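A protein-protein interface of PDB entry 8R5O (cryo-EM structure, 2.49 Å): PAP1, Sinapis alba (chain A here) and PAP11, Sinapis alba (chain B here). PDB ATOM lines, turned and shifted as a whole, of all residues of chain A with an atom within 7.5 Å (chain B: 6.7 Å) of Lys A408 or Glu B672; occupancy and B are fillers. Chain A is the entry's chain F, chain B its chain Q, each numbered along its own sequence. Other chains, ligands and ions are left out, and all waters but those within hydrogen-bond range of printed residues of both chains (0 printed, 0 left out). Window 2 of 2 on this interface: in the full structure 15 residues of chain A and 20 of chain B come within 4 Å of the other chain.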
ATOM      1  N   MET A 405     -12.383  -4.344  -9.867  1.00  0.00           N
ATOM      2  CA  MET A 405     -11.884  -4.864  -8.605  1.00  0.00           C
ATOM      3  C   MET A 405     -11.116  -6.157  -8.841  1.00  0.00           C
ATOM      4  O   MET A 405     -11.544  -7.011  -9.624  1.00  0.00           O
ATOM      5  CB  MET A 405     -13.039  -5.100  -7.632  1.00  0.00           C
ATOM      6  CG  MET A 405     -12.621  -5.321  -6.197  1.00  0.00           C
ATOM      7  SD  MET A 405     -14.011  -5.106  -5.074  1.00  0.00           S
ATOM      8  CE  MET A 405     -15.236  -6.152  -5.855  1.00  0.00           C
ATOM      9  N   SER A 406      -9.981  -6.296  -8.162  1.00  0.00           N
ATOM     10  CA  SER A 406      -9.144  -7.474  -8.308  1.00  0.00           C
ATOM     11  C   SER A 406      -9.641  -8.597  -7.399  1.00  0.00           C
ATOM     12  O   SER A 406     -10.640  -8.464  -6.686  1.00  0.00           O
ATOM     13  CB  SER A 406      -7.687  -7.130  -8.009  1.00  0.00           C
ATOM     14  OG  SER A 406      -7.533  -6.667  -6.680  1.00  0.00           O
ATOM     15  N   ARG A 407      -8.931  -9.728  -7.431  1.00  0.00           N
ATOM     16  CA  ARG A 407      -9.303 -10.862  -6.590  1.00  0.00           C
ATOM     17  C   ARG A 407      -9.189 -10.520  -5.111  1.00  0.00           C
ATOM     18  O   ARG A 407     -10.059 -10.886  -4.312  1.00  0.00           O
ATOM     19  CB  ARG A 407      -8.433 -12.073  -6.918  1.00  0.00           C
ATOM     20  CG  ARG A 407      -8.983 -12.942  -8.024  1.00  0.00           C
ATOM     21  CD  ARG A 407      -8.617 -14.396  -7.802  1.00  0.00           C
ATOM     22  NE  ARG A 407      -9.005 -14.855  -6.474  1.00  0.00           N
ATOM     23  CZ  ARG A 407      -8.154 -15.136  -5.497  1.00  0.00           C
ATOM     24  NH1 ARG A 407      -6.847 -15.036  -5.669  1.00  0.00           N
ATOM     25  NH2 ARG A 407      -8.627 -15.531  -4.318  1.00  0.00           N
ATOM     26  N   LYS A 408      -8.125  -9.822  -4.726  1.00  0.00           N
ATOM     27  CA  LYS A 408      -7.920  -9.427  -3.341  1.00  0.00           C
ATOM     28  C   LYS A 408      -8.778  -8.237  -2.937  1.00  0.00           C
ATOM     29  O   LYS A 408      -8.541  -7.653  -1.874  1.00  0.00           O
ATOM     30  CB  LYS A 408      -6.441  -9.116  -3.100  1.00  0.00           C
ATOM     31  CG  LYS A 408      -5.501 -10.221  -3.558  1.00  0.00           C
ATOM     32  CD  LYS A 408      -5.903 -11.567  -2.976  1.00  0.00           C
ATOM     33  CE  LYS A 408      -5.097 -12.701  -3.586  1.00  0.00           C
ATOM     34  NZ  LYS A 408      -3.649 -12.603  -3.259  1.00  0.00           N
ATOM     35  N   TYR A 409      -9.757  -7.870  -3.765  1.00  0.00           N
ATOM     36  CA  TYR A 409     -10.696  -6.785  -3.485  1.00  0.00           C
ATOM     37  C   TYR A 409      -9.963  -5.460  -3.272  1.00  0.00           C
ATOM     38  O   TYR A 409     -10.080  -4.804  -2.236  1.00  0.00           O
ATOM     39  CB  TYR A 409     -11.595  -7.137  -2.297  1.00  0.00           C
ATOM     40  CG  TYR A 409     -12.755  -8.021  -2.688  1.00  0.00           C
ATOM     41  CD1 TYR A 409     -12.547  -9.322  -3.121  1.00  0.00           C
ATOM     42  CD2 TYR A 409     -14.058  -7.550  -2.635  1.00  0.00           C
ATOM     43  CE1 TYR A 409     -13.602 -10.130  -3.488  1.00  0.00           C
ATOM     44  CE2 TYR A 409     -15.121  -8.351  -2.998  1.00  0.00           C
ATOM     45  CZ  TYR A 409     -14.887  -9.640  -3.423  1.00  0.00           C
ATOM     46  OH  TYR A 409     -15.946 -10.441  -3.785  1.00  0.00           O
ATOM     47  N   ARG A 410      -9.195  -5.080  -4.290  1.00  0.00           N
ATOM     48  CA  ARG A 410      -8.516  -3.797  -4.335  1.00  0.00           C
ATOM     49  C   ARG A 410      -8.763  -3.148  -5.688  1.00  0.00           C
ATOM     50  O   ARG A 410      -8.915  -3.830  -6.705  1.00  0.00           O
ATOM     51  CB  ARG A 410      -7.009  -3.942  -4.084  1.00  0.00           C
ATOM     52  CG  ARG A 410      -6.660  -4.403  -2.681  1.00  0.00           C
ATOM     53  CD  ARG A 410      -5.293  -3.896  -2.254  1.00  0.00           C
ATOM     54  NE  ARG A 410      -4.203  -4.769  -2.672  1.00  0.00           N
ATOM     55  CZ  ARG A 410      -2.925  -4.417  -2.679  1.00  0.00           C
ATOM     56  NH1 ARG A 410      -2.542  -3.197  -2.344  1.00  0.00           N
ATOM     57  NH2 ARG A 410      -2.008  -5.310  -3.038  1.00  0.00           N
ATOM     58  N   THR A 411      -8.801  -1.822  -5.690  1.00  0.00           N
ATOM     59  CA  THR A 411      -9.051  -1.026  -6.884  1.00  0.00           C
ATOM     60  C   THR A 411      -7.820  -0.171  -7.179  1.00  0.00           C
ATOM     61  O   THR A 411      -6.765  -0.332  -6.558  1.00  0.00           O
ATOM     62  CB  THR A 411     -10.309  -0.171  -6.710  1.00  0.00           C
ATOM     63  OG1 THR A 411     -10.125   0.737  -5.620  1.00  0.00           O
ATOM     64  CG2 THR A 411     -11.514  -1.048  -6.426  1.00  0.00           C
ATOM     65  N   LEU A 420       2.051  -6.613  -3.218  1.00  0.00           N
ATOM     66  CA  LEU A 420       1.217  -6.695  -4.407  1.00  0.00           C
ATOM     67  C   LEU A 420       0.387  -7.972  -4.409  1.00  0.00           C
ATOM     68  O   LEU A 420       0.852  -9.040  -4.000  1.00  0.00           O
ATOM     69  CB  LEU A 420       2.065  -6.621  -5.678  1.00  0.00           C
ATOM     70  CG  LEU A 420       2.621  -5.243  -6.045  1.00  0.00           C
ATOM     71  CD1 LEU A 420       3.272  -5.272  -7.418  1.00  0.00           C
ATOM     72  CD2 LEU A 420       1.530  -4.187  -5.990  1.00  0.00           C
ATOM     73  N   GLN A 421      -0.855  -7.843  -4.878  1.00  0.00           N
ATOM     74  CA  GLN A 421      -1.799  -8.958  -4.965  1.00  0.00           C
ATOM     75  C   GLN A 421      -2.019  -9.622  -3.610  1.00  0.00           C
ATOM     76  O   GLN A 421      -2.233 -10.833  -3.528  1.00  0.00           O
ATOM     77  CB  GLN A 421      -1.347  -9.991  -6.001  1.00  0.00           C
ATOM     78  CG  GLN A 421      -1.255  -9.453  -7.420  1.00  0.00           C
ATOM     79  CD  GLN A 421      -2.613  -9.135  -8.015  1.00  0.00           C
ATOM     80  OE1 GLN A 421      -3.638  -9.643  -7.561  1.00  0.00           O
ATOM     81  NE2 GLN A 421      -2.626  -8.290  -9.038  1.00  0.00           N
ATOM     82  N   GLU A 422      -1.958  -8.839  -2.536  1.00  0.00           N
ATOM     83  CA  GLU A 422      -2.162  -9.339  -1.185  1.00  0.00           C
ATOM     84  C   GLU A 422      -3.143  -8.439  -0.453  1.00  0.00           C
ATOM     85  O   GLU A 422      -3.149  -7.220  -0.652  1.00  0.00           O
ATOM     86  CB  GLU A 422      -0.844  -9.410  -0.406  1.00  0.00           C
ATOM     87  CG  GLU A 422       0.211 -10.300  -1.038  1.00  0.00           C
ATOM     88  CD  GLU A 422       1.431 -10.471  -0.156  1.00  0.00           C
ATOM     89  OE1 GLU A 422       1.278 -10.429   1.083  1.00  0.00           O
ATOM     90  OE2 GLU A 422       2.542 -10.644  -0.699  1.00  0.00           O
ATOM     91  N   GLU A 423      -3.970  -9.045   0.393  1.00  0.00           N
ATOM     92  CA  GLU A 423      -4.932  -8.297   1.183  1.00  0.00           C
ATOM     93  C   GLU A 423      -4.254  -7.670   2.400  1.00  0.00           C
ATOM     94  O   GLU A 423      -3.060  -7.858   2.650  1.00  0.00           O
ATOM     95  CB  GLU A 423      -6.081  -9.202   1.619  1.00  0.00           C
ATOM     96  CG  GLU A 423      -6.740  -9.956   0.481  1.00  0.00           C
ATOM     97  CD  GLU A 423      -8.245  -9.783   0.461  1.00  0.00           C
ATOM     98  OE1 GLU A 423      -8.740  -8.796   1.047  1.00  0.00           O
ATOM     99  OE2 GLU A 423      -8.934 -10.635  -0.137  1.00  0.00           O
ATOM    100  N   ALA A 424      -5.033  -6.914   3.161  1.00  0.00           N
ATOM    101  CA  ALA A 424      -4.566  -6.261   4.373  1.00  0.00           C
ATOM    102  C   ALA A 424      -5.184  -6.937   5.595  1.00  0.00           C
ATOM    103  O   ALA A 424      -6.009  -7.846   5.484  1.00  0.00           O
ATOM    104  CB  ALA A 424      -4.887  -4.767   4.337  1.00  0.00           C
ATOM    105  N   LEU A 426      -7.123  -5.765   8.261  1.00  0.00           N
ATOM    106  CA  LEU A 426      -8.532  -5.435   8.477  1.00  0.00           C
ATOM    107  C   LEU A 426      -8.980  -5.644   9.920  1.00  0.00           C
ATOM    108  O   LEU A 426     -10.115  -5.307  10.270  1.00  0.00           O
ATOM    109  CB  LEU A 426      -9.435  -6.244   7.541  1.00  0.00           C
ATOM    110  CG  LEU A 426      -9.430  -5.871   6.061  1.00  0.00           C
ATOM    111  CD1 LEU A 426     -10.426  -6.725   5.298  1.00  0.00           C
ATOM    112  CD2 LEU A 426      -9.747  -4.400   5.894  1.00  0.00           C
ATOM    113  N   ILE A 430     -11.447 -12.467   7.072  1.00  0.00           N
ATOM    114  CA  ILE A 430     -12.312 -12.191   5.933  1.00  0.00           C
ATOM    115  C   ILE A 430     -13.379 -13.272   5.830  1.00  0.00           C
ATOM    116  O   ILE A 430     -13.085 -14.470   5.934  1.00  0.00           O
ATOM    117  CB  ILE A 430     -11.486 -12.105   4.642  1.00  0.00           C
ATOM    118  CG1 ILE A 430     -10.453 -10.984   4.743  1.00  0.00           C
ATOM    119  CG2 ILE A 430     -12.391 -11.898   3.442  1.00  0.00           C
ATOM    120  CD1 ILE A 430      -9.525 -10.911   3.557  1.00  0.00           C
ATOM    121  N   TYR A 432     -15.165 -15.273   3.600  1.00  0.00           N
ATOM    122  CA  TYR A 432     -15.130 -15.712   2.212  1.00  0.00           C
ATOM    123  C   TYR A 432     -16.466 -16.263   1.735  1.00  0.00           C
ATOM    124  O   TYR A 432     -16.701 -16.310   0.524  1.00  0.00           O
ATOM    125  CB  TYR A 432     -14.042 -16.767   2.021  1.00  0.00           C
ATOM    126  CG  TYR A 432     -12.643 -16.247   2.249  1.00  0.00           C
ATOM    127  CD1 TYR A 432     -12.045 -15.389   1.339  1.00  0.00           C
ATOM    128  CD2 TYR A 432     -11.915 -16.622   3.368  1.00  0.00           C
ATOM    129  CE1 TYR A 432     -10.768 -14.913   1.538  1.00  0.00           C
ATOM    130  CE2 TYR A 432     -10.635 -16.153   3.576  1.00  0.00           C
ATOM    131  CZ  TYR A 432     -10.066 -15.298   2.658  1.00  0.00           C
ATOM    132  OH  TYR A 432      -8.790 -14.826   2.859  1.00  0.00           O
ATOM    133  N   ARG A 435     -18.348 -13.228   0.362  1.00  0.00           N
ATOM    134  CA  ARG A 435     -17.875 -12.909  -0.981  1.00  0.00           C
ATOM    135  C   ARG A 435     -18.420 -13.893  -2.004  1.00  0.00           C
ATOM    136  O   ARG A 435     -18.746 -13.510  -3.133  1.00  0.00           O
ATOM    137  CB  ARG A 435     -16.348 -12.897  -1.012  1.00  0.00           C
ATOM    138  CG  ARG A 435     -15.721 -11.748  -0.252  1.00  0.00           C
ATOM    139  CD  ARG A 435     -14.208 -11.790  -0.352  1.00  0.00           C
ATOM    140  NE  ARG A 435     -13.586 -10.638   0.288  1.00  0.00           N
ATOM    141  CZ  ARG A 435     -12.280 -10.418   0.320  1.00  0.00           C
ATOM    142  NH1 ARG A 435     -11.424 -11.254  -0.242  1.00  0.00           N
ATOM    143  NH2 ARG A 435     -11.820  -9.331   0.934  1.00  0.00           N
ATOM    144  N   TRP A 449     -12.043 -18.690 -11.731  1.00  0.00           N
ATOM    145  CA  TRP A 449     -10.654 -18.428 -12.102  1.00  0.00           C
ATOM    146  C   TRP A 449      -9.931 -19.732 -12.432  1.00  0.00           C
ATOM    147  O   TRP A 449      -8.919 -20.090 -11.833  1.00  0.00           O
ATOM    148  CB  TRP A 449      -9.949 -17.661 -10.989  1.00  0.00           C
ATOM    149  CG  TRP A 449     -10.506 -16.289 -10.789  1.00  0.00           C
ATOM    150  CD1 TRP A 449     -11.649 -15.960 -10.126  1.00  0.00           C
ATOM    151  CD2 TRP A 449      -9.947 -15.060 -11.263  1.00  0.00           C
ATOM    152  NE1 TRP A 449     -11.838 -14.601 -10.155  1.00  0.00           N
ATOM    153  CE2 TRP A 449     -10.806 -14.024 -10.848  1.00  0.00           C
ATOM    154  CE3 TRP A 449      -8.803 -14.735 -11.997  1.00  0.00           C
ATOM    155  CZ2 TRP A 449     -10.558 -12.686 -11.142  1.00  0.00           C
ATOM    156  CZ3 TRP A 449      -8.558 -13.405 -12.288  1.00  0.00           C
ATOM    157  CH2 TRP A 449      -9.431 -12.397 -11.861  1.00  0.00           C
ATOM    158  N   PRO A 451      -7.993 -21.679 -15.388  1.00  0.00           N
ATOM    159  CA  PRO A 451      -7.365 -21.521 -16.705  1.00  0.00           C
ATOM    160  C   PRO A 451      -7.940 -22.504 -17.714  1.00  0.00           C
ATOM    161  O   PRO A 451      -8.214 -23.663 -17.395  1.00  0.00           O
ATOM    162  CB  PRO A 451      -5.884 -21.803 -16.427  1.00  0.00           C
ATOM    163  CG  PRO A 451      -5.718 -21.575 -14.959  1.00  0.00           C
ATOM    164  CD  PRO A 451      -7.011 -21.998 -14.341  1.00  0.00           C
ATOM    165  N   THR A 810     -12.680   0.264  -1.763  1.00  0.00           N
ATOM    166  CA  THR A 810     -13.100  -0.871  -0.959  1.00  0.00           C
ATOM    167  C   THR A 810     -12.551  -0.765   0.462  1.00  0.00           C
ATOM    168  O   THR A 810     -11.684   0.056   0.769  1.00  0.00           O
ATOM    169  CB  THR A 810     -12.641  -2.180  -1.596  1.00  0.00           C
ATOM    170  OG1 THR A 810     -11.210  -2.218  -1.635  1.00  0.00           O
ATOM    171  CG2 THR A 810     -13.179  -2.297  -3.006  1.00  0.00           C
ATOM    172  N   GLY A 812     -10.770  -3.078   1.797  1.00  0.00           N
ATOM    173  CA  GLY A 812      -9.383  -3.494   1.683  1.00  0.00           C
ATOM    174  C   GLY A 812      -8.470  -2.371   1.229  1.00  0.00           C
ATOM    175  O   GLY A 812      -7.318  -2.285   1.662  1.00  0.00           O
ATOM    176  N   ASP A 813      -8.965  -1.500   0.347  1.00  0.00           N
ATOM    177  CA  ASP A 813      -8.159  -0.374  -0.113  1.00  0.00           C
ATOM    178  C   ASP A 813      -7.811   0.564   1.033  1.00  0.00           C
ATOM    179  O   ASP A 813      -6.678   1.050   1.125  1.00  0.00           O
ATOM    180  CB  ASP A 813      -8.890   0.389  -1.216  1.00  0.00           C
ATOM    181  CG  ASP A 813      -8.799  -0.300  -2.559  1.00  0.00           C
ATOM    182  OD1 ASP A 813      -7.769  -0.954  -2.824  1.00  0.00           O
ATOM    183  OD2 ASP A 813      -9.756  -0.185  -3.351  1.00  0.00           O
ATOM    184  N   VAL A 816      -5.048  -0.922   3.166  1.00  0.00           N
ATOM    185  CA  VAL A 816      -3.748  -0.941   2.504  1.00  0.00           C
ATOM    186  C   VAL A 816      -3.093   0.434   2.563  1.00  0.00           C
ATOM    187  O   VAL A 816      -1.885   0.551   2.799  1.00  0.00           O
ATOM    188  CB  VAL A 816      -3.894  -1.443   1.057  1.00  0.00           C
ATOM    189  CG1 VAL A 816      -2.622  -1.191   0.277  1.00  0.00           C
ATOM    190  CG2 VAL A 816      -4.231  -2.920   1.049  1.00  0.00           C
ATOM    191  N   GLY B 667     -10.029 -18.629   0.299  1.00  0.00           N
ATOM    192  CA  GLY B 667      -9.314 -17.545  -0.342  1.00  0.00           C
ATOM    193  C   GLY B 667      -8.415 -17.940  -1.489  1.00  0.00           C
ATOM    194  O   GLY B 667      -7.557 -17.143  -1.882  1.00  0.00           O
ATOM    195  N   TRP B 668      -8.578 -19.137  -2.039  1.00  0.00           N
ATOM    196  CA  TRP B 668      -7.752 -19.614  -3.137  1.00  0.00           C
ATOM    197  C   TRP B 668      -8.553 -19.655  -4.431  1.00  0.00           C
ATOM    198  O   TRP B 668      -9.774 -19.489  -4.450  1.00  0.00           O
ATOM    199  CB  TRP B 668      -7.182 -21.004  -2.836  1.00  0.00           C
ATOM    200  CG  TRP B 668      -6.094 -21.019  -1.815  1.00  0.00           C
ATOM    201  CD1 TRP B 668      -5.945 -20.170  -0.761  1.00  0.00           C
ATOM    202  CD2 TRP B 668      -4.988 -21.926  -1.758  1.00  0.00           C
ATOM    203  NE1 TRP B 668      -4.819 -20.495  -0.046  1.00  0.00           N
ATOM    204  CE2 TRP B 668      -4.213 -21.572  -0.639  1.00  0.00           C
ATOM    205  CE3 TRP B 668      -4.580 -23.008  -2.546  1.00  0.00           C
ATOM    206  CZ2 TRP B 668      -3.055 -22.258  -0.285  1.00  0.00           C
ATOM    207  CZ3 TRP B 668      -3.430 -23.689  -2.193  1.00  0.00           C
ATOM    208  CH2 TRP B 668      -2.680 -23.310  -1.073  1.00  0.00           C
ATOM    209  N   THR B 669      -7.833 -19.882  -5.526  1.00  0.00           N
ATOM    210  CA  THR B 669      -8.431 -20.108  -6.831  1.00  0.00           C
ATOM    211  C   THR B 669      -7.679 -21.233  -7.521  1.00  0.00           C
ATOM    212  O   THR B 669      -6.552 -21.569  -7.153  1.00  0.00           O
ATOM    213  CB  THR B 669      -8.419 -18.846  -7.705  1.00  0.00           C
ATOM    214  OG1 THR B 669      -7.171 -18.160  -7.548  1.00  0.00           O
ATOM    215  CG2 THR B 669      -9.563 -17.923  -7.324  1.00  0.00           C
ATOM    216  N   MET B 670      -8.326 -21.825  -8.526  1.00  0.00           N
ATOM    217  CA  MET B 670      -7.700 -22.922  -9.255  1.00  0.00           C
ATOM    218  C   MET B 670      -6.417 -22.467  -9.938  1.00  0.00           C
ATOM    219  O   MET B 670      -5.437 -23.217  -9.996  1.00  0.00           O
ATOM    220  CB  MET B 670      -8.678 -23.500 -10.276  1.00  0.00           C
ATOM    221  CG  MET B 670      -8.116 -24.662 -11.075  1.00  0.00           C
ATOM    222  SD  MET B 670      -7.634 -26.056 -10.040  1.00  0.00           S
ATOM    223  CE  MET B 670      -9.223 -26.556  -9.388  1.00  0.00           C
ATOM    224  N   GLN B 671      -6.404 -21.236 -10.453  1.00  0.00           N
ATOM    225  CA  GLN B 671      -5.213 -20.720 -11.115  1.00  0.00           C
ATOM    226  C   GLN B 671      -4.035 -20.628 -10.154  1.00  0.00           C
ATOM    227  O   GLN B 671      -2.906 -20.991 -10.507  1.00  0.00           O
ATOM    228  CB  GLN B 671      -5.510 -19.353 -11.730  1.00  0.00           C
ATOM    229  CG  GLN B 671      -4.335 -18.732 -12.457  1.00  0.00           C
ATOM    230  CD  GLN B 671      -4.643 -17.350 -12.985  1.00  0.00           C
ATOM    231  OE1 GLN B 671      -4.725 -17.141 -14.195  1.00  0.00           O
ATOM    232  NE2 GLN B 671      -4.814 -16.396 -12.079  1.00  0.00           N
ATOM    233  N   GLU B 672      -4.275 -20.141  -8.934  1.00  0.00           N
ATOM    234  CA  GLU B 672      -3.199 -20.047  -7.952  1.00  0.00           C
ATOM    235  C   GLU B 672      -2.695 -21.426  -7.547  1.00  0.00           C
ATOM    236  O   GLU B 672      -1.488 -21.627  -7.370  1.00  0.00           O
ATOM    237  CB  GLU B 672      -3.669 -19.266  -6.726  1.00  0.00           C
ATOM    238  CG  GLU B 672      -3.973 -17.806  -7.003  1.00  0.00           C
ATOM    239  CD  GLU B 672      -4.349 -17.043  -5.750  1.00  0.00           C
ATOM    240  OE1 GLU B 672      -4.384 -17.660  -4.665  1.00  0.00           O
ATOM    241  OE2 GLU B 672      -4.608 -15.825  -5.851  1.00  0.00           O
ATOM    242  N   TYR B 673      -3.607 -22.388  -7.384  1.00  0.00           N
ATOM    243  CA  TYR B 673      -3.189 -23.745  -7.047  1.00  0.00           C
ATOM    244  C   TYR B 673      -2.359 -24.360  -8.166  1.00  0.00           C
ATOM    245  O   TYR B 673      -1.357 -25.035  -7.907  1.00  0.00           O
ATOM    246  CB  TYR B 673      -4.410 -24.615  -6.746  1.00  0.00           C
ATOM    247  CG  TYR B 673      -4.060 -26.045  -6.404  1.00  0.00           C
ATOM    248  CD1 TYR B 673      -3.703 -26.401  -5.110  1.00  0.00           C
ATOM    249  CD2 TYR B 673      -4.080 -27.038  -7.372  1.00  0.00           C
ATOM    250  CE1 TYR B 673      -3.377 -27.703  -4.792  1.00  0.00           C
ATOM    251  CE2 TYR B 673      -3.755 -28.342  -7.063  1.00  0.00           C
ATOM    252  CZ  TYR B 673      -3.405 -28.669  -5.773  1.00  0.00           C
ATOM    253  OH  TYR B 673      -3.084 -29.969  -5.465  1.00  0.00           O
ATOM    254  N   LEU B 674      -2.763 -24.142  -9.419  1.00  0.00           N
ATOM    255  CA  LEU B 674      -2.011 -24.687 -10.542  1.00  0.00           C
ATOM    256  C   LEU B 674      -0.652 -24.017 -10.687  1.00  0.00           C
ATOM    257  O   LEU B 674       0.303 -24.654 -11.144  1.00  0.00           O
ATOM    258  CB  LEU B 674      -2.819 -24.551 -11.830  1.00  0.00           C
ATOM    259  CG  LEU B 674      -4.095 -25.389 -11.899  1.00  0.00           C
ATOM    260  CD1 LEU B 674      -4.843 -25.132 -13.195  1.00  0.00           C
ATOM    261  CD2 LEU B 674      -3.773 -26.864 -11.746  1.00  0.00           C
ATOM    262  N   LYS B 675      -0.543 -22.738 -10.319  1.00  0.00           N
ATOM    263  CA  LYS B 675       0.760 -22.080 -10.321  1.00  0.00           C
ATOM    264  C   LYS B 675       1.697 -22.722  -9.308  1.00  0.00           C
ATOM    265  O   LYS B 675       2.889 -22.904  -9.583  1.00  0.00           O
ATOM    266  CB  LYS B 675       0.604 -20.588 -10.036  1.00  0.00           C
ATOM    267  CG  LYS B 675       0.260 -19.755 -11.256  1.00  0.00           C
ATOM    268  CD  LYS B 675       0.209 -18.275 -10.917  1.00  0.00           C
ATOM    269  CE  LYS B 675       0.101 -17.425 -12.173  1.00  0.00           C
ATOM    270  NZ  LYS B 675      -1.098 -17.769 -12.982  1.00  0.00           N
ATOM    271  N   HIS B 676       1.179 -23.065  -8.126  1.00  0.00           N
ATOM    272  CA  HIS B 676       1.990 -23.767  -7.139  1.00  0.00           C
ATOM    273  C   HIS B 676       2.419 -25.137  -7.642  1.00  0.00           C
ATOM    274  O   HIS B 676       3.487 -25.630  -7.264  1.00  0.00           O
ATOM    275  CB  HIS B 676       1.221 -23.899  -5.825  1.00  0.00           C
ATOM    276  CG  HIS B 676       1.055 -22.607  -5.089  1.00  0.00           C
ATOM    277  ND1 HIS B 676       2.038 -21.642  -5.049  1.00  0.00           N
ATOM    278  CD2 HIS B 676       0.018 -22.117  -4.370  1.00  0.00           C
ATOM    279  CE1 HIS B 676       1.615 -20.615  -4.333  1.00  0.00           C
ATOM    280  NE2 HIS B 676       0.392 -20.878  -3.910  1.00  0.00           N
ATOM    281  N   GLY B 677       1.601 -25.770  -8.484  1.00  0.00           N
ATOM    282  CA  GLY B 677       1.992 -27.044  -9.064  1.00  0.00           C
ATOM    283  C   GLY B 677       3.169 -26.918 -10.012  1.00  0.00           C
ATOM    284  O   GLY B 677       4.009 -27.818 -10.096  1.00  0.00           O
ATOM    285  N   TYR B 682       3.298 -26.927  -2.925  1.00  0.00           N
ATOM    286  CA  TYR B 682       2.045 -26.355  -2.468  1.00  0.00           C
ATOM    287  C   TYR B 682       2.207 -25.881  -1.035  1.00  0.00           C
ATOM    288  O   TYR B 682       2.436 -26.713  -0.143  1.00  0.00           O
ATOM    289  CB  TYR B 682       0.922 -27.380  -2.562  1.00  0.00           C
ATOM    290  CG  TYR B 682       0.751 -27.962  -3.944  1.00  0.00           C
ATOM    291  CD1 TYR B 682       0.065 -27.271  -4.930  1.00  0.00           C
ATOM    292  CD2 TYR B 682       1.275 -29.206  -4.263  1.00  0.00           C
ATOM    293  CE1 TYR B 682      -0.094 -27.798  -6.193  1.00  0.00           C
ATOM    294  CE2 TYR B 682       1.120 -29.742  -5.524  1.00  0.00           C
ATOM    295  CZ  TYR B 682       0.435 -29.034  -6.484  1.00  0.00           C
ATOM    296  OH  TYR B 682       0.278 -29.565  -7.742  1.00  0.00           O
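The guanidinium group (NH1) of Arg A407 is in salt-bridge range of the side-chain carboxylate (OE1) of Glu B672 (3.7 Å). O of Gly B667 lies within hydrogen-bond range of NH2 of Arg A407 (3.1 Å). The backbone NH (N) of Gln B671 lies within hydrogen-bond range of the backbone carbonyl oxygen (O) of Trp A449 (3.1 Å).
Among the printed residues, merely in contact across the chains: Arg A407 with Thr B669 (3.2 Å), Tyr A432 with Gly B667 (3.5 Å), Trp A449 with Thr B669 (3.7 Å), Trp A449 with Met B670 (3.8 Å), Lys A408 with Glu B672 (3.9 Å), Pro A451 with Gln B671 (3.9 Å) and Pro A451 with Leu B674 (3.98 Å).
Of the printed residues of chain B, Lys A408 touches Glu B672 (3.9 Å). Printed residues of chain B within 4 Å of Tyr A432: Gly B667 (3.5 Å). Of the printed residues of chain B, Trp A449 touches Thr B669 (3.7 Å), Met B670 (3.8 Å) and Gln B671 (3.1 Å). Val A816 touches none of the printed residues of chain B. Of chain A, only Arg A407 and Lys A408 come within 4 Å of Glu B672. The nearest residue of chain A that does not touch Glu B672 is Trp A449 (5.5 Å).
Hydrophobic or aromatic side chains of chain B within 4 Å of the printed part of chain A: Met B670 and Leu B674. Of the 22 printed residues of chain A, 5 touch a printed residue of chain B. Hydrophobic or aromatic side chains of chain A within 4 Å of the printed part of chain B: Tyr A432, Trp A449 and Pro A451. Among the printed residues, 10 pairs touch across the chains. Among the printed residues, Asp or Glu carboxylates within 4 Å of a Lys or Arg side-chain nitrogen of the other chain: Arg A407 with Glu B672.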
